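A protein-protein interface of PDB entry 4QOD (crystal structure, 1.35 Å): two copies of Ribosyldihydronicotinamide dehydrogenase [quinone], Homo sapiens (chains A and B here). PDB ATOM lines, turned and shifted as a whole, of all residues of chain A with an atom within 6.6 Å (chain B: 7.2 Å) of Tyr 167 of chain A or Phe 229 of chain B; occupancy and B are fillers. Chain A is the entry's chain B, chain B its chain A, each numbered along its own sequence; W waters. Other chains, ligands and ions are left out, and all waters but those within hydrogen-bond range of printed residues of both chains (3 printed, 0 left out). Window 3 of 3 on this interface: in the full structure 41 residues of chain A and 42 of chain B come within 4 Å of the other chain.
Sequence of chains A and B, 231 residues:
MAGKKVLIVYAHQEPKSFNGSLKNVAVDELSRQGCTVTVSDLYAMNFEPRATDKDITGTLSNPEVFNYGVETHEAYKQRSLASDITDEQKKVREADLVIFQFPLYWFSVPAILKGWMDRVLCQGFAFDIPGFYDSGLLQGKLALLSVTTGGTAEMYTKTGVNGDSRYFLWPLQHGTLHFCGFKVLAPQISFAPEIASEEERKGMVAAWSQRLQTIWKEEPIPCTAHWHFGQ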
ATOM      1  N   PHE A 107     -21.300  -3.521 -27.854  1.00  0.00           N
ATOM      2  CA  PHE A 107     -21.376  -4.943 -27.478  1.00  0.00           C
ATOM      3  C   PHE A 107     -20.271  -5.771 -28.084  1.00  0.00           C
ATOM      4  O   PHE A 107     -20.452  -6.980 -28.253  1.00  0.00           O
ATOM      5  CB  PHE A 107     -22.754  -5.632 -27.811  1.00  0.00           C
ATOM      6  CG  PHE A 107     -23.874  -5.366 -26.805  1.00  0.00           C
ATOM      7  CD1 PHE A 107     -23.920  -4.256 -25.995  1.00  0.00           C
ATOM      8  CD2 PHE A 107     -24.941  -6.353 -26.696  1.00  0.00           C
ATOM      9  CE1 PHE A 107     -24.980  -3.996 -25.144  1.00  0.00           C
ATOM     10  CE2 PHE A 107     -26.004  -6.087 -25.853  1.00  0.00           C
ATOM     11  CZ  PHE A 107     -26.004  -4.952 -25.053  1.00  0.00           C
ATOM     12  N   THR A 157     -27.343  -8.217 -16.617  1.00  0.00           N
ATOM     13  CA  THR A 157     -28.010  -9.417 -16.155  1.00  0.00           C
ATOM     14  C   THR A 157     -29.117  -9.787 -17.083  1.00  0.00           C
ATOM     15  O   THR A 157     -29.570  -8.958 -17.844  1.00  0.00           O
ATOM     16  CB  THR A 157     -28.600  -9.239 -14.783  1.00  0.00           C
ATOM     17  OG1 THR A 157     -29.316  -8.011 -14.746  1.00  0.00           O
ATOM     18  CG2 THR A 157     -27.503  -9.200 -13.768  1.00  0.00           C
ATOM     19  N   LYS A 158     -29.534 -11.040 -17.004  1.00  0.00           N
ATOM     20  CA  LYS A 158     -30.398 -11.749 -17.981  1.00  0.00           C
ATOM     21  C   LYS A 158     -31.640 -10.939 -18.344  1.00  0.00           C
ATOM     22  O   LYS A 158     -32.072 -10.894 -19.506  1.00  0.00           O
ATOM     23  CB  LYS A 158     -30.909 -13.087 -17.403  1.00  0.00           C
ATOM     24  CG  LYS A 158     -29.869 -14.187 -17.159  1.00  0.00           C
ATOM     25  CD  LYS A 158     -29.636 -15.069 -18.382  1.00  0.00           C
ATOM     26  CE  LYS A 158     -29.042 -16.415 -18.008  1.00  0.00           C
ATOM     27  NZ  LYS A 158     -28.821 -17.275 -19.212  1.00  0.00           N
ATOM     28  N   THR A 159     -32.211 -10.337 -17.313  1.00  0.00           N
ATOM     29  CA  THR A 159     -33.430  -9.556 -17.416  1.00  0.00           C
ATOM     30  C   THR A 159     -33.067  -8.063 -17.297  1.00  0.00           C
ATOM     31  O   THR A 159     -33.935  -7.190 -17.117  1.00  0.00           O
ATOM     32  CB  THR A 159     -34.414  -9.959 -16.287  1.00  0.00           C
ATOM     33  OG1 THR A 159     -33.826  -9.701 -14.987  1.00  0.00           O
ATOM     34  CG2 THR A 159     -34.805 -11.459 -16.429  1.00  0.00           C
ATOM     35  N   ASN A 162     -29.445  -4.739 -21.049  1.00  0.00           N
ATOM     36  CA  ASN A 162     -28.377  -5.191 -21.881  1.00  0.00           C
ATOM     37  C   ASN A 162     -28.289  -6.676 -21.983  1.00  0.00           C
ATOM     38  O   ASN A 162     -27.620  -7.134 -22.918  1.00  0.00           O
ATOM     39  CB  ASN A 162     -26.984  -4.595 -21.528  1.00  0.00           C
ATOM     40  CG  ASN A 162     -26.887  -3.073 -21.622  1.00  0.00           C
ATOM     41  OD1 ASN A 162     -27.542  -2.374 -22.459  1.00  0.00           O
ATOM     42  ND2 ASN A 162     -25.980  -2.500 -20.806  1.00  0.00           N
ATOM     43  N   GLY A 163     -29.077  -7.416 -21.135  1.00  0.00           N
ATOM     44  CA  GLY A 163     -28.932  -8.844 -21.115  1.00  0.00           C
ATOM     45  C   GLY A 163     -27.641  -9.173 -20.390  1.00  0.00           C
ATOM     46  O   GLY A 163     -26.884  -8.250 -19.960  1.00  0.00           O
ATOM     47  N   ASP A 164     -27.440 -10.474 -20.234  1.00  0.00           N
ATOM     48  CA  ASP A 164     -26.271 -11.014 -19.581  1.00  0.00           C
ATOM     49  C   ASP A 164     -25.005 -10.648 -20.409  1.00  0.00           C
ATOM     50  O   ASP A 164     -25.012 -10.809 -21.589  1.00  0.00           O
ATOM     51  CB  ASP A 164     -26.494 -12.560 -19.477  1.00  0.00           C
ATOM     52  CG  ASP A 164     -25.470 -13.309 -18.573  1.00  0.00           C
ATOM     53  OD1 ASP A 164     -24.433 -12.778 -18.225  1.00  0.00           O
ATOM     54  OD2 ASP A 164     -25.731 -14.495 -18.259  1.00  0.00           O
ATOM     55  N   SER A 165     -23.903 -10.305 -19.730  1.00  0.00           N
ATOM     56  CA  SER A 165     -22.655 -10.061 -20.397  1.00  0.00           C
ATOM     57  C   SER A 165     -22.268 -11.299 -21.233  1.00  0.00           C
ATOM     58  O   SER A 165     -21.604 -11.223 -22.304  1.00  0.00           O
ATOM     59  CB  SER A 165     -21.541  -9.596 -19.400  1.00  0.00           C
ATOM     60  OG  SER A 165     -21.464 -10.504 -18.330  1.00  0.00           O
ATOM     61  N   ARG A 166     -22.569 -12.505 -20.776  1.00  0.00           N
ATOM     62  CA  ARG A 166     -22.205 -13.621 -21.577  1.00  0.00           C
ATOM     63  C   ARG A 166     -22.763 -13.590 -23.001  1.00  0.00           C
ATOM     64  O   ARG A 166     -22.229 -14.226 -23.912  1.00  0.00           O
ATOM     65  CB  ARG A 166     -22.560 -14.967 -20.884  1.00  0.00           C
ATOM     66  CG  ARG A 166     -21.775 -15.176 -19.579  1.00  0.00           C
ATOM     67  CD  ARG A 166     -21.984 -16.567 -19.008  1.00  0.00           C
ATOM     68  NE  ARG A 166     -21.278 -16.705 -17.729  1.00  0.00           N
ATOM     69  CZ  ARG A 166     -21.140 -17.886 -17.094  1.00  0.00           C
ATOM     70  NH1 ARG A 166     -21.536 -19.037 -17.682  1.00  0.00           N
ATOM     71  NH2 ARG A 166     -20.517 -17.945 -15.930  1.00  0.00           N
ATOM     72  N   TYR A 167     -23.943 -12.995 -23.152  1.00  0.00           N
ATOM     73  CA  TYR A 167     -24.601 -12.993 -24.449  1.00  0.00           C
ATOM     74  C   TYR A 167     -23.746 -12.308 -25.507  1.00  0.00           C
ATOM     75  O   TYR A 167     -23.574 -12.861 -26.593  1.00  0.00           O
ATOM     76  CB  TYR A 167     -25.956 -12.276 -24.361  1.00  0.00           C
ATOM     77  CG  TYR A 167     -27.004 -12.953 -23.516  1.00  0.00           C
ATOM     78  CD1 TYR A 167     -26.867 -14.301 -23.027  1.00  0.00           C
ATOM     79  CD2 TYR A 167     -28.143 -12.206 -23.108  1.00  0.00           C
ATOM     80  CE1 TYR A 167     -27.934 -14.885 -22.281  1.00  0.00           C
ATOM     81  CE2 TYR A 167     -29.170 -12.773 -22.425  1.00  0.00           C
ATOM     82  CZ  TYR A 167     -29.052 -14.096 -21.949  1.00  0.00           C
ATOM     83  OH  TYR A 167     -30.139 -14.573 -21.205  1.00  0.00           O
ATOM     84  N   PHE A 168     -23.109 -11.166 -25.150  1.00  0.00           N
ATOM     85  CA  PHE A 168     -22.282 -10.449 -26.114  1.00  0.00           C
ATOM     86  C   PHE A 168     -20.909 -11.089 -26.243  1.00  0.00           C
ATOM     87  O   PHE A 168     -20.194 -10.858 -27.241  1.00  0.00           O
ATOM     88  CB  PHE A 168     -22.247  -8.944 -25.816  1.00  0.00           C
ATOM     89  CG  PHE A 168     -21.398  -8.559 -24.614  1.00  0.00           C
ATOM     90  CD1 PHE A 168     -20.003  -8.835 -24.569  1.00  0.00           C
ATOM     91  CD2 PHE A 168     -22.006  -7.921 -23.554  1.00  0.00           C
ATOM     92  CE1 PHE A 168     -19.269  -8.498 -23.452  1.00  0.00           C
ATOM     93  CE2 PHE A 168     -21.277  -7.500 -22.474  1.00  0.00           C
ATOM     94  CZ  PHE A 168     -19.896  -7.801 -22.418  1.00  0.00           C
ATOM     95  N   LEU A 169     -20.508 -11.947 -25.298  1.00  0.00           N
ATOM     96  CA  LEU A 169     -19.226 -12.644 -25.475  1.00  0.00           C
ATOM     97  C   LEU A 169     -19.196 -13.682 -26.538  1.00  0.00           C
ATOM     98  O   LEU A 169     -18.167 -14.064 -27.026  1.00  0.00           O
ATOM     99  CB  LEU A 169     -18.732 -13.267 -24.145  1.00  0.00           C
ATOM    100  CG  LEU A 169     -18.477 -12.258 -23.016  1.00  0.00           C
ATOM    101  CD1 LEU A 169     -18.285 -12.990 -21.676  1.00  0.00           C
ATOM    102  CD2 LEU A 169     -17.218 -11.415 -23.315  1.00  0.00           C
ATOM    103  N   TRP A 170     -20.383 -14.212 -26.886  1.00  0.00           N
ATOM    104  CA  TRP A 170     -20.433 -15.281 -27.841  1.00  0.00           C
ATOM    105  C   TRP A 170     -19.655 -15.148 -29.123  1.00  0.00           C
ATOM    106  O   TRP A 170     -18.880 -16.018 -29.550  1.00  0.00           O
ATOM    107  CB  TRP A 170     -21.944 -15.667 -28.045  1.00  0.00           C
ATOM    108  CG  TRP A 170     -22.236 -16.676 -29.033  1.00  0.00           C
ATOM    109  CD1 TRP A 170     -22.872 -16.533 -30.261  1.00  0.00           C
ATOM    110  CD2 TRP A 170     -22.111 -18.103 -28.836  1.00  0.00           C
ATOM    111  NE1 TRP A 170     -23.039 -17.778 -30.888  1.00  0.00           N
ATOM    112  CE2 TRP A 170     -22.581 -18.747 -30.030  1.00  0.00           C
ATOM    113  CE3 TRP A 170     -21.605 -18.897 -27.778  1.00  0.00           C
ATOM    114  CZ2 TRP A 170     -22.615 -20.143 -30.172  1.00  0.00           C
ATOM    115  CZ3 TRP A 170     -21.585 -20.282 -27.947  1.00  0.00           C
ATOM    116  CH2 TRP A 170     -22.079 -20.889 -29.134  1.00  0.00           C
ATOM    117  N   PRO A 171     -19.865 -14.011 -29.872  1.00  0.00           N
ATOM    118  CA  PRO A 171     -19.135 -13.918 -31.118  1.00  0.00           C
ATOM    119  C   PRO A 171     -17.577 -13.815 -30.959  1.00  0.00           C
ATOM    120  O   PRO A 171     -16.903 -14.264 -31.804  1.00  0.00           O
ATOM    121  CB  PRO A 171     -19.619 -12.564 -31.735  1.00  0.00           C
ATOM    122  CG  PRO A 171     -20.998 -12.447 -31.132  1.00  0.00           C
ATOM    123  CD  PRO A 171     -20.877 -12.938 -29.707  1.00  0.00           C
ATOM    124  N   HIS A 228     -22.825 -19.717 -22.380  1.00  0.00           N
ATOM    125  CA  HIS A 228     -23.197 -18.311 -22.701  1.00  0.00           C
ATOM    126  C   HIS A 228     -24.687 -17.903 -22.450  1.00  0.00           C
ATOM    127  O   HIS A 228     -24.993 -16.805 -21.944  1.00  0.00           O
ATOM    128  CB  HIS A 228     -22.784 -18.072 -24.154  1.00  0.00           C
ATOM    129  CG  HIS A 228     -21.289 -18.015 -24.340  1.00  0.00           C
ATOM    130  ND1 HIS A 228     -20.530 -19.130 -24.626  1.00  0.00           N
ATOM    131  CD2 HIS A 228     -20.436 -16.945 -24.440  1.00  0.00           C
ATOM    132  CE1 HIS A 228     -19.264 -18.776 -24.799  1.00  0.00           C
ATOM    133  NE2 HIS A 228     -19.198 -17.448 -24.744  1.00  0.00           N
ATOM    134  N   PHE A 229     -25.575 -18.898 -22.578  1.00  0.00           N
ATOM    135  CA  PHE A 229     -27.013 -18.692 -22.772  1.00  0.00           C
ATOM    136  C   PHE A 229     -27.849 -19.474 -21.802  1.00  0.00           C
ATOM    137  O   PHE A 229     -28.994 -19.080 -21.602  1.00  0.00           O
ATOM    138  CB  PHE A 229     -27.487 -19.038 -24.241  1.00  0.00           C
ATOM    139  CG  PHE A 229     -26.670 -18.362 -25.316  1.00  0.00           C
ATOM    140  CD1 PHE A 229     -26.562 -16.974 -25.307  1.00  0.00           C
ATOM    141  CD2 PHE A 229     -26.057 -19.084 -26.342  1.00  0.00           C
ATOM    142  CE1 PHE A 229     -25.793 -16.320 -26.264  1.00  0.00           C
ATOM    143  CE2 PHE A 229     -25.301 -18.420 -27.300  1.00  0.00           C
ATOM    144  CZ  PHE A 229     -25.194 -17.037 -27.248  1.00  0.00           C
ATOM    145  N   GLY A 230     -27.312 -20.547 -21.201  1.00  0.00           N
ATOM    146  CA  GLY A 230     -28.141 -21.449 -20.316  1.00  0.00           C
ATOM    147  C   GLY A 230     -28.273 -21.044 -18.829  1.00  0.00           C
ATOM    148  O   GLY A 230     -27.782 -19.989 -18.436  1.00  0.00           O
ATOM    149  N   LYS B 158     -29.298 -24.386 -33.612  1.00  0.00           N
ATOM    150  CA  LYS B 158     -28.992 -24.590 -32.206  1.00  0.00           C
ATOM    151  C   LYS B 158     -28.061 -25.771 -32.061  1.00  0.00           C
ATOM    152  O   LYS B 158     -27.130 -25.701 -31.288  1.00  0.00           O
ATOM    153  CB  LYS B 158     -30.270 -24.809 -31.443  1.00  0.00           C
ATOM    154  CG  LYS B 158     -30.109 -24.864 -29.956  1.00  0.00           C
ATOM    155  CD  LYS B 158     -31.284 -25.597 -29.336  1.00  0.00           C
ATOM    156  CE  LYS B 158     -31.339 -25.373 -27.843  1.00  0.00           C
ATOM    157  NZ  LYS B 158     -32.147 -24.165 -27.550  1.00  0.00           N
ATOM    158  N   ASP B 164     -27.213 -21.221 -33.113  1.00  0.00           N
ATOM    159  CA  ASP B 164     -28.249 -20.539 -33.889  1.00  0.00           C
ATOM    160  C   ASP B 164     -27.770 -19.213 -34.452  1.00  0.00           C
ATOM    161  O   ASP B 164     -27.166 -18.415 -33.715  1.00  0.00           O
ATOM    162  CB  ASP B 164     -29.525 -20.321 -33.122  1.00  0.00           C
ATOM    163  CG  ASP B 164     -30.657 -20.084 -34.081  1.00  0.00           C
ATOM    164  OD1 ASP B 164     -30.958 -20.974 -34.952  1.00  0.00           O
ATOM    165  OD2 ASP B 164     -31.120 -18.995 -34.088  1.00  0.00           O
ATOM    166  N   ARG B 166     -29.444 -16.529 -34.812  1.00  0.00           N
ATOM    167  CA  ARG B 166     -29.916 -15.440 -33.959  1.00  0.00           C
ATOM    168  C   ARG B 166     -28.955 -15.051 -32.859  1.00  0.00           C
ATOM    169  O   ARG B 166     -28.937 -13.881 -32.408  1.00  0.00           O
ATOM    170  CB  ARG B 166     -31.316 -15.665 -33.396  1.00  0.00           C
ATOM    171  CG  ARG B 166     -32.380 -15.810 -34.459  1.00  0.00           C
ATOM    172  CD  ARG B 166     -33.730 -15.894 -33.758  1.00  0.00           C
ATOM    173  NE  ARG B 166     -34.795 -16.001 -34.785  1.00  0.00           N
ATOM    174  CZ  ARG B 166     -36.076 -16.015 -34.483  1.00  0.00           C
ATOM    175  NH1 ARG B 166     -36.512 -15.780 -33.260  1.00  0.00           N
ATOM    176  NH2 ARG B 166     -36.999 -15.987 -35.439  1.00  0.00           N
ATOM    177  N   TYR B 167     -28.141 -16.031 -32.443  1.00  0.00           N
ATOM    178  CA  TYR B 167     -27.277 -15.754 -31.306  1.00  0.00           C
ATOM    179  C   TYR B 167     -26.263 -14.638 -31.638  1.00  0.00           C
ATOM    180  O   TYR B 167     -26.020 -13.765 -30.744  1.00  0.00           O
ATOM    181  CB  TYR B 167     -26.467 -16.980 -30.835  1.00  0.00           C
ATOM    182  CG  TYR B 167     -27.273 -18.170 -30.324  1.00  0.00           C
ATOM    183  CD1 TYR B 167     -28.583 -18.047 -29.964  1.00  0.00           C
ATOM    184  CD2 TYR B 167     -26.635 -19.384 -30.119  1.00  0.00           C
ATOM    185  CE1 TYR B 167     -29.314 -19.150 -29.494  1.00  0.00           C
ATOM    186  CE2 TYR B 167     -27.328 -20.485 -29.608  1.00  0.00           C
ATOM    187  CZ  TYR B 167     -28.645 -20.348 -29.299  1.00  0.00           C
ATOM    188  OH  TYR B 167     -29.291 -21.427 -28.807  1.00  0.00           O
ATOM    189  N   PHE B 168     -25.706 -14.672 -32.862  1.00  0.00           N
ATOM    190  CA  PHE B 168     -24.698 -13.671 -33.243  1.00  0.00           C
ATOM    191  C   PHE B 168     -25.320 -12.360 -33.633  1.00  0.00           C
ATOM    192  O   PHE B 168     -24.652 -11.331 -33.705  1.00  0.00           O
ATOM    193  CB  PHE B 168     -23.726 -14.278 -34.280  1.00  0.00           C
ATOM    194  CG  PHE B 168     -24.275 -14.468 -35.675  1.00  0.00           C
ATOM    195  CD1 PHE B 168     -24.785 -13.446 -36.446  1.00  0.00           C
ATOM    196  CD2 PHE B 168     -24.311 -15.789 -36.224  1.00  0.00           C
ATOM    197  CE1 PHE B 168     -25.268 -13.689 -37.757  1.00  0.00           C
ATOM    198  CE2 PHE B 168     -24.782 -16.028 -37.496  1.00  0.00           C
ATOM    199  CZ  PHE B 168     -25.278 -14.992 -38.254  1.00  0.00           C
ATOM    200  N   LEU B 169     -26.616 -12.365 -33.844  1.00  0.00           N
ATOM    201  CA  LEU B 169     -27.294 -11.086 -34.196  1.00  0.00           C
ATOM    202  C   LEU B 169     -27.489 -10.148 -33.049  1.00  0.00           C
ATOM    203  O   LEU B 169     -27.634  -8.920 -33.249  1.00  0.00           O
ATOM    204  CB  LEU B 169     -28.644 -11.309 -34.871  1.00  0.00           C
ATOM    205  CG  LEU B 169     -28.666 -12.138 -36.124  1.00  0.00           C
ATOM    206  CD1 LEU B 169     -30.108 -12.431 -36.518  1.00  0.00           C
ATOM    207  CD2 LEU B 169     -27.945 -11.440 -37.241  1.00  0.00           C
ATOM    208  N   TRP B 170     -27.372 -10.625 -31.827  1.00  0.00           N
ATOM    209  CA  TRP B 170     -27.676  -9.863 -30.682  1.00  0.00           C
ATOM    210  C   TRP B 170     -26.862  -8.548 -30.540  1.00  0.00           C
ATOM    211  O   TRP B 170     -27.475  -7.517 -30.280  1.00  0.00           O
ATOM    212  CB  TRP B 170     -27.543 -10.785 -29.406  1.00  0.00           C
ATOM    213  CG  TRP B 170     -27.648 -10.133 -28.098  1.00  0.00           C
ATOM    214  CD1 TRP B 170     -26.625  -9.957 -27.122  1.00  0.00           C
ATOM    215  CD2 TRP B 170     -28.841  -9.735 -27.444  1.00  0.00           C
ATOM    216  NE1 TRP B 170     -27.158  -9.408 -25.990  1.00  0.00           N
ATOM    217  CE2 TRP B 170     -28.520  -9.340 -26.117  1.00  0.00           C
ATOM    218  CE3 TRP B 170     -30.193  -9.764 -27.824  1.00  0.00           C
ATOM    219  CZ2 TRP B 170     -29.484  -8.844 -25.225  1.00  0.00           C
ATOM    220  CZ3 TRP B 170     -31.121  -9.275 -26.941  1.00  0.00           C
ATOM    221  CH2 TRP B 170     -30.806  -8.899 -25.630  1.00  0.00           C
ATOM    222  N   PRO B 171     -25.497  -8.572 -30.635  1.00  0.00           N
ATOM    223  CA  PRO B 171     -24.786  -7.317 -30.513  1.00  0.00           C
ATOM    224  C   PRO B 171     -25.167  -6.250 -31.521  1.00  0.00           C
ATOM    225  O   PRO B 171     -25.097  -5.063 -31.243  1.00  0.00           O
ATOM    226  CB  PRO B 171     -23.302  -7.711 -30.625  1.00  0.00           C
ATOM    227  CG  PRO B 171     -23.282  -9.143 -30.276  1.00  0.00           C
ATOM    228  CD  PRO B 171     -24.599  -9.711 -30.781  1.00  0.00           C
ATOM    229  N   THR B 224     -35.750  -8.619 -28.479  1.00  0.00           N
ATOM    230  CA  THR B 224     -35.638  -8.988 -27.082  1.00  0.00           C
ATOM    231  C   THR B 224     -34.691 -10.198 -26.960  1.00  0.00           C
ATOM    232  O   THR B 224     -34.396 -10.952 -27.886  1.00  0.00           O
ATOM    233  CB  THR B 224     -37.049  -9.424 -26.577  1.00  0.00           C
ATOM    234  OG1 THR B 224     -37.446 -10.600 -27.267  1.00  0.00           O
ATOM    235  CG2 THR B 224     -38.086  -8.302 -26.707  1.00  0.00           C
ATOM    236  N   ALA B 225     -34.285 -10.389 -25.707  1.00  0.00           N
ATOM    237  CA  ALA B 225     -33.503 -11.557 -25.365  1.00  0.00           C
ATOM    238  C   ALA B 225     -34.231 -12.870 -25.740  1.00  0.00           C
ATOM    239  O   ALA B 225     -33.682 -13.805 -26.338  1.00  0.00           O
ATOM    240  CB  ALA B 225     -33.113 -11.541 -23.911  1.00  0.00           C
ATOM    241  N   HIS B 226     -35.558 -12.861 -25.470  1.00  0.00           N
ATOM    242  CA  HIS B 226     -36.343 -14.075 -25.819  1.00  0.00           C
ATOM    243  C   HIS B 226     -36.270 -14.442 -27.325  1.00  0.00           C
ATOM    244  O   HIS B 226     -36.044 -15.549 -27.772  1.00  0.00           O
ATOM    245  CB  HIS B 226     -37.779 -13.976 -25.331  1.00  0.00           C
ATOM    246  CG  HIS B 226     -38.524 -15.251 -25.578  1.00  0.00           C
ATOM    247  ND1 HIS B 226     -39.346 -15.450 -26.666  1.00  0.00           N
ATOM    248  CD2 HIS B 226     -38.436 -16.447 -24.962  1.00  0.00           C
ATOM    249  CE1 HIS B 226     -39.807 -16.697 -26.655  1.00  0.00           C
ATOM    250  NE2 HIS B 226     -39.273 -17.319 -25.631  1.00  0.00           N
ATOM    251  N   TRP B 227     -36.459 -13.391 -28.155  1.00  0.00           N
ATOM    252  CA  TRP B 227     -36.349 -13.631 -29.564  1.00  0.00           C
ATOM    253  C   TRP B 227     -35.033 -14.203 -30.021  1.00  0.00           C
ATOM    254  O   TRP B 227     -34.991 -15.130 -30.822  1.00  0.00           O
ATOM    255  CB  TRP B 227     -36.688 -12.319 -30.358  1.00  0.00           C
ATOM    256  CG  TRP B 227     -36.780 -12.498 -31.841  1.00  0.00           C
ATOM    257  CD1 TRP B 227     -37.939 -12.707 -32.590  1.00  0.00           C
ATOM    258  CD2 TRP B 227     -35.725 -12.427 -32.814  1.00  0.00           C
ATOM    259  NE1 TRP B 227     -37.664 -12.810 -33.923  1.00  0.00           N
ATOM    260  CE2 TRP B 227     -36.302 -12.587 -34.092  1.00  0.00           C
ATOM    261  CE3 TRP B 227     -34.342 -12.206 -32.724  1.00  0.00           C
ATOM    262  CZ2 TRP B 227     -35.540 -12.640 -35.277  1.00  0.00           C
ATOM    263  CZ3 TRP B 227     -33.607 -12.306 -33.924  1.00  0.00           C
ATOM    264  CH2 TRP B 227     -34.191 -12.489 -35.161  1.00  0.00           C
ATOM    265  N   HIS B 228     -33.916 -13.669 -29.442  1.00  0.00           N
ATOM    266  CA  HIS B 228     -32.616 -14.102 -29.916  1.00  0.00           C
ATOM    267  C   HIS B 228     -32.186 -15.470 -29.335  1.00  0.00           C
ATOM    268  O   HIS B 228     -31.545 -16.252 -30.054  1.00  0.00           O
ATOM    269  CB  HIS B 228     -31.601 -13.036 -29.515  1.00  0.00           C
ATOM    270  CG  HIS B 228     -31.658 -11.783 -30.335  1.00  0.00           C
ATOM    271  ND1 HIS B 228     -32.522 -10.749 -30.063  1.00  0.00           N
ATOM    272  CD2 HIS B 228     -30.927 -11.410 -31.424  1.00  0.00           C
ATOM    273  CE1 HIS B 228     -32.341  -9.771 -30.969  1.00  0.00           C
ATOM    274  NE2 HIS B 228     -31.398 -10.168 -31.820  1.00  0.00           N
ATOM    275  N   PHE B 229     -32.614 -15.725 -28.073  1.00  0.00           N
ATOM    276  CA  PHE B 229     -32.050 -16.887 -27.320  1.00  0.00           C
ATOM    277  C   PHE B 229     -33.044 -17.953 -26.886  1.00  0.00           C
ATOM    278  O   PHE B 229     -32.644 -19.064 -26.566  1.00  0.00           O
ATOM    279  CB  PHE B 229     -31.248 -16.385 -26.102  1.00  0.00           C
ATOM    280  CG  PHE B 229     -30.238 -15.351 -26.466  1.00  0.00           C
ATOM    281  CD1 PHE B 229     -29.198 -15.652 -27.340  1.00  0.00           C
ATOM    282  CD2 PHE B 229     -30.361 -14.094 -25.928  1.00  0.00           C
ATOM    283  CE1 PHE B 229     -28.269 -14.643 -27.692  1.00  0.00           C
ATOM    284  CE2 PHE B 229     -29.385 -13.101 -26.266  1.00  0.00           C
ATOM    285  CZ  PHE B 229     -28.411 -13.428 -27.174  1.00  0.00           C
ATOM    286  N   GLY B 230     -34.328 -17.612 -26.876  1.00  0.00           N
ATOM    287  CA  GLY B 230     -35.355 -18.569 -26.363  1.00  0.00           C
ATOM    288  C   GLY B 230     -35.495 -18.463 -24.873  1.00  0.00           C
ATOM    289  O   GLY B 230     -35.027 -17.501 -24.251  1.00  0.00           O
ATOM    290  N   GLN B 231     -36.233 -19.441 -24.289  1.00  0.00           N
ATOM    291  CA  GLN B 231     -36.776 -19.360 -22.899  1.00  0.00           C
ATOM    292  C   GLN B 231     -35.831 -19.404 -21.732  1.00  0.00           C
ATOM    293  O   GLN B 231     -36.244 -19.852 -20.645  1.00  0.00           O
HETATM  294  O   HOH W   1     -25.707  -8.823 -23.558  1.00  0.00           O
HETATM  295  O   HOH W   2     -24.407 -18.549 -33.334  1.00  0.00           O
HETATM  296  O   HOH W   3     -24.121 -12.574 -29.156  1.00  0.00           O
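O of Phe 229 of chain A sits at hydrogen-bond distance from NZ of Lys 158 of chain A (3.0 Å).
Tyr 167 of chain A touches Trp 170 of chain B, and with the chains exchanged Trp 170 of chain A touches Tyr 167 of chain B. Tyr 167 of chain A touches Phe 229 of chain B, and with the chains exchanged Phe 229 of chain A touches Tyr 167 of chain B. Phe 229 of chain B touches its own counterpart, Phe 229 of chain A.
Water W1 lies within hydrogen-bond range of O of Asn 162 of chain A, O of Asp 164 of chain A and NE1 of Trp 170 of chain B. Water W3 lies within hydrogen-bond range of the backbone carbonyl oxygen (O) of Tyr 167 of chain A and the backbone carbonyl oxygen (O) of Tyr 167 of chain B. Water W2 lies within hydrogen-bond range of O of Asp 164 of chain B and NE1 of Trp 170 of chain A.
Printed residues of chain B within 4 Å of Phe 107 of chain A: Trp 170 (3.5 Å) and Pro 171 (3.5 Å). Printed residues of chain B within 4 Å of Asn 162 of chain A: Trp 170 (3.4 Å). Of chain B, only Trp 170 (3.5 Å) and Phe 229 (3.5 Å) come within 4 Å of Tyr 167 of chain A. His 228 of chain A touches none of the printed residues of chain B. Printed residues of chain A within 4 Å of Tyr 167 of chain B: Trp 170 (3.5 Å) and Phe 229 (3.3 Å). Of the printed residues of chain A, Trp 170 of chain B touches Phe 107, Asn 162 and Tyr 167. Of the printed residues of chain A, Pro 171 of chain B touches Phe 107 (3.5 Å). Phe 229 of chain B touches just these residues of chain A: Tyr 167 (3.5 Å) and Phe 229 (3.3 Å). Gly 230 of chain B touches none of the printed residues of chain A. The nearest printed residue of chain B that does not touch Asn 162 of chain A is Phe 229 of chain B (7.1 Å).
Phe 107 of chain A touches Trp 170 of chain B (CE2 to NE1, 3.5 Å). Pro 171 of chain B touches Phe 107 of chain A (CB to CB, 3.5 Å). O of Asn 162 of chain A touches CZ2 of Trp 170 of chain B, at 3.4 Å. Trp 170 of chain B touches Tyr 167 of chain A (NE1 to CB, 3.5 Å). CD2 of Tyr 167 of chain A touches CE2 of Phe 229 of chain B, at 3.5 Å. Trp 170 of chain A touches Tyr 167 of chain B. CE2 of Phe 229 of chain A touches CD2 of Tyr 167 of chain B, at 3.3 Å. Phe 229 of chain A touches Phe 229 of chain B.
Of the 17 printed residues of chain A, 5 touch a printed residue of chain B. Hydrophobic or aromatic side chains of chain A within 4 Å of the printed part of chain B: Phe 107, Tyr 167, Trp 170 and Phe 229. Along chain A the printed residues that touch a printed residue of chain B span positions 107 to 229. Hydrophobic or aromatic side chains of chain B within 4 Å of the printed part of chain A: Tyr 167, Trp 170, Pro 171 and Phe 229. Among the printed residues, 8 pairs touch across the chains. Among the printed residues, no Asp or Glu carboxylate lies within 4 Å of a Lys or Arg side-chain nitrogen of the other chain.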
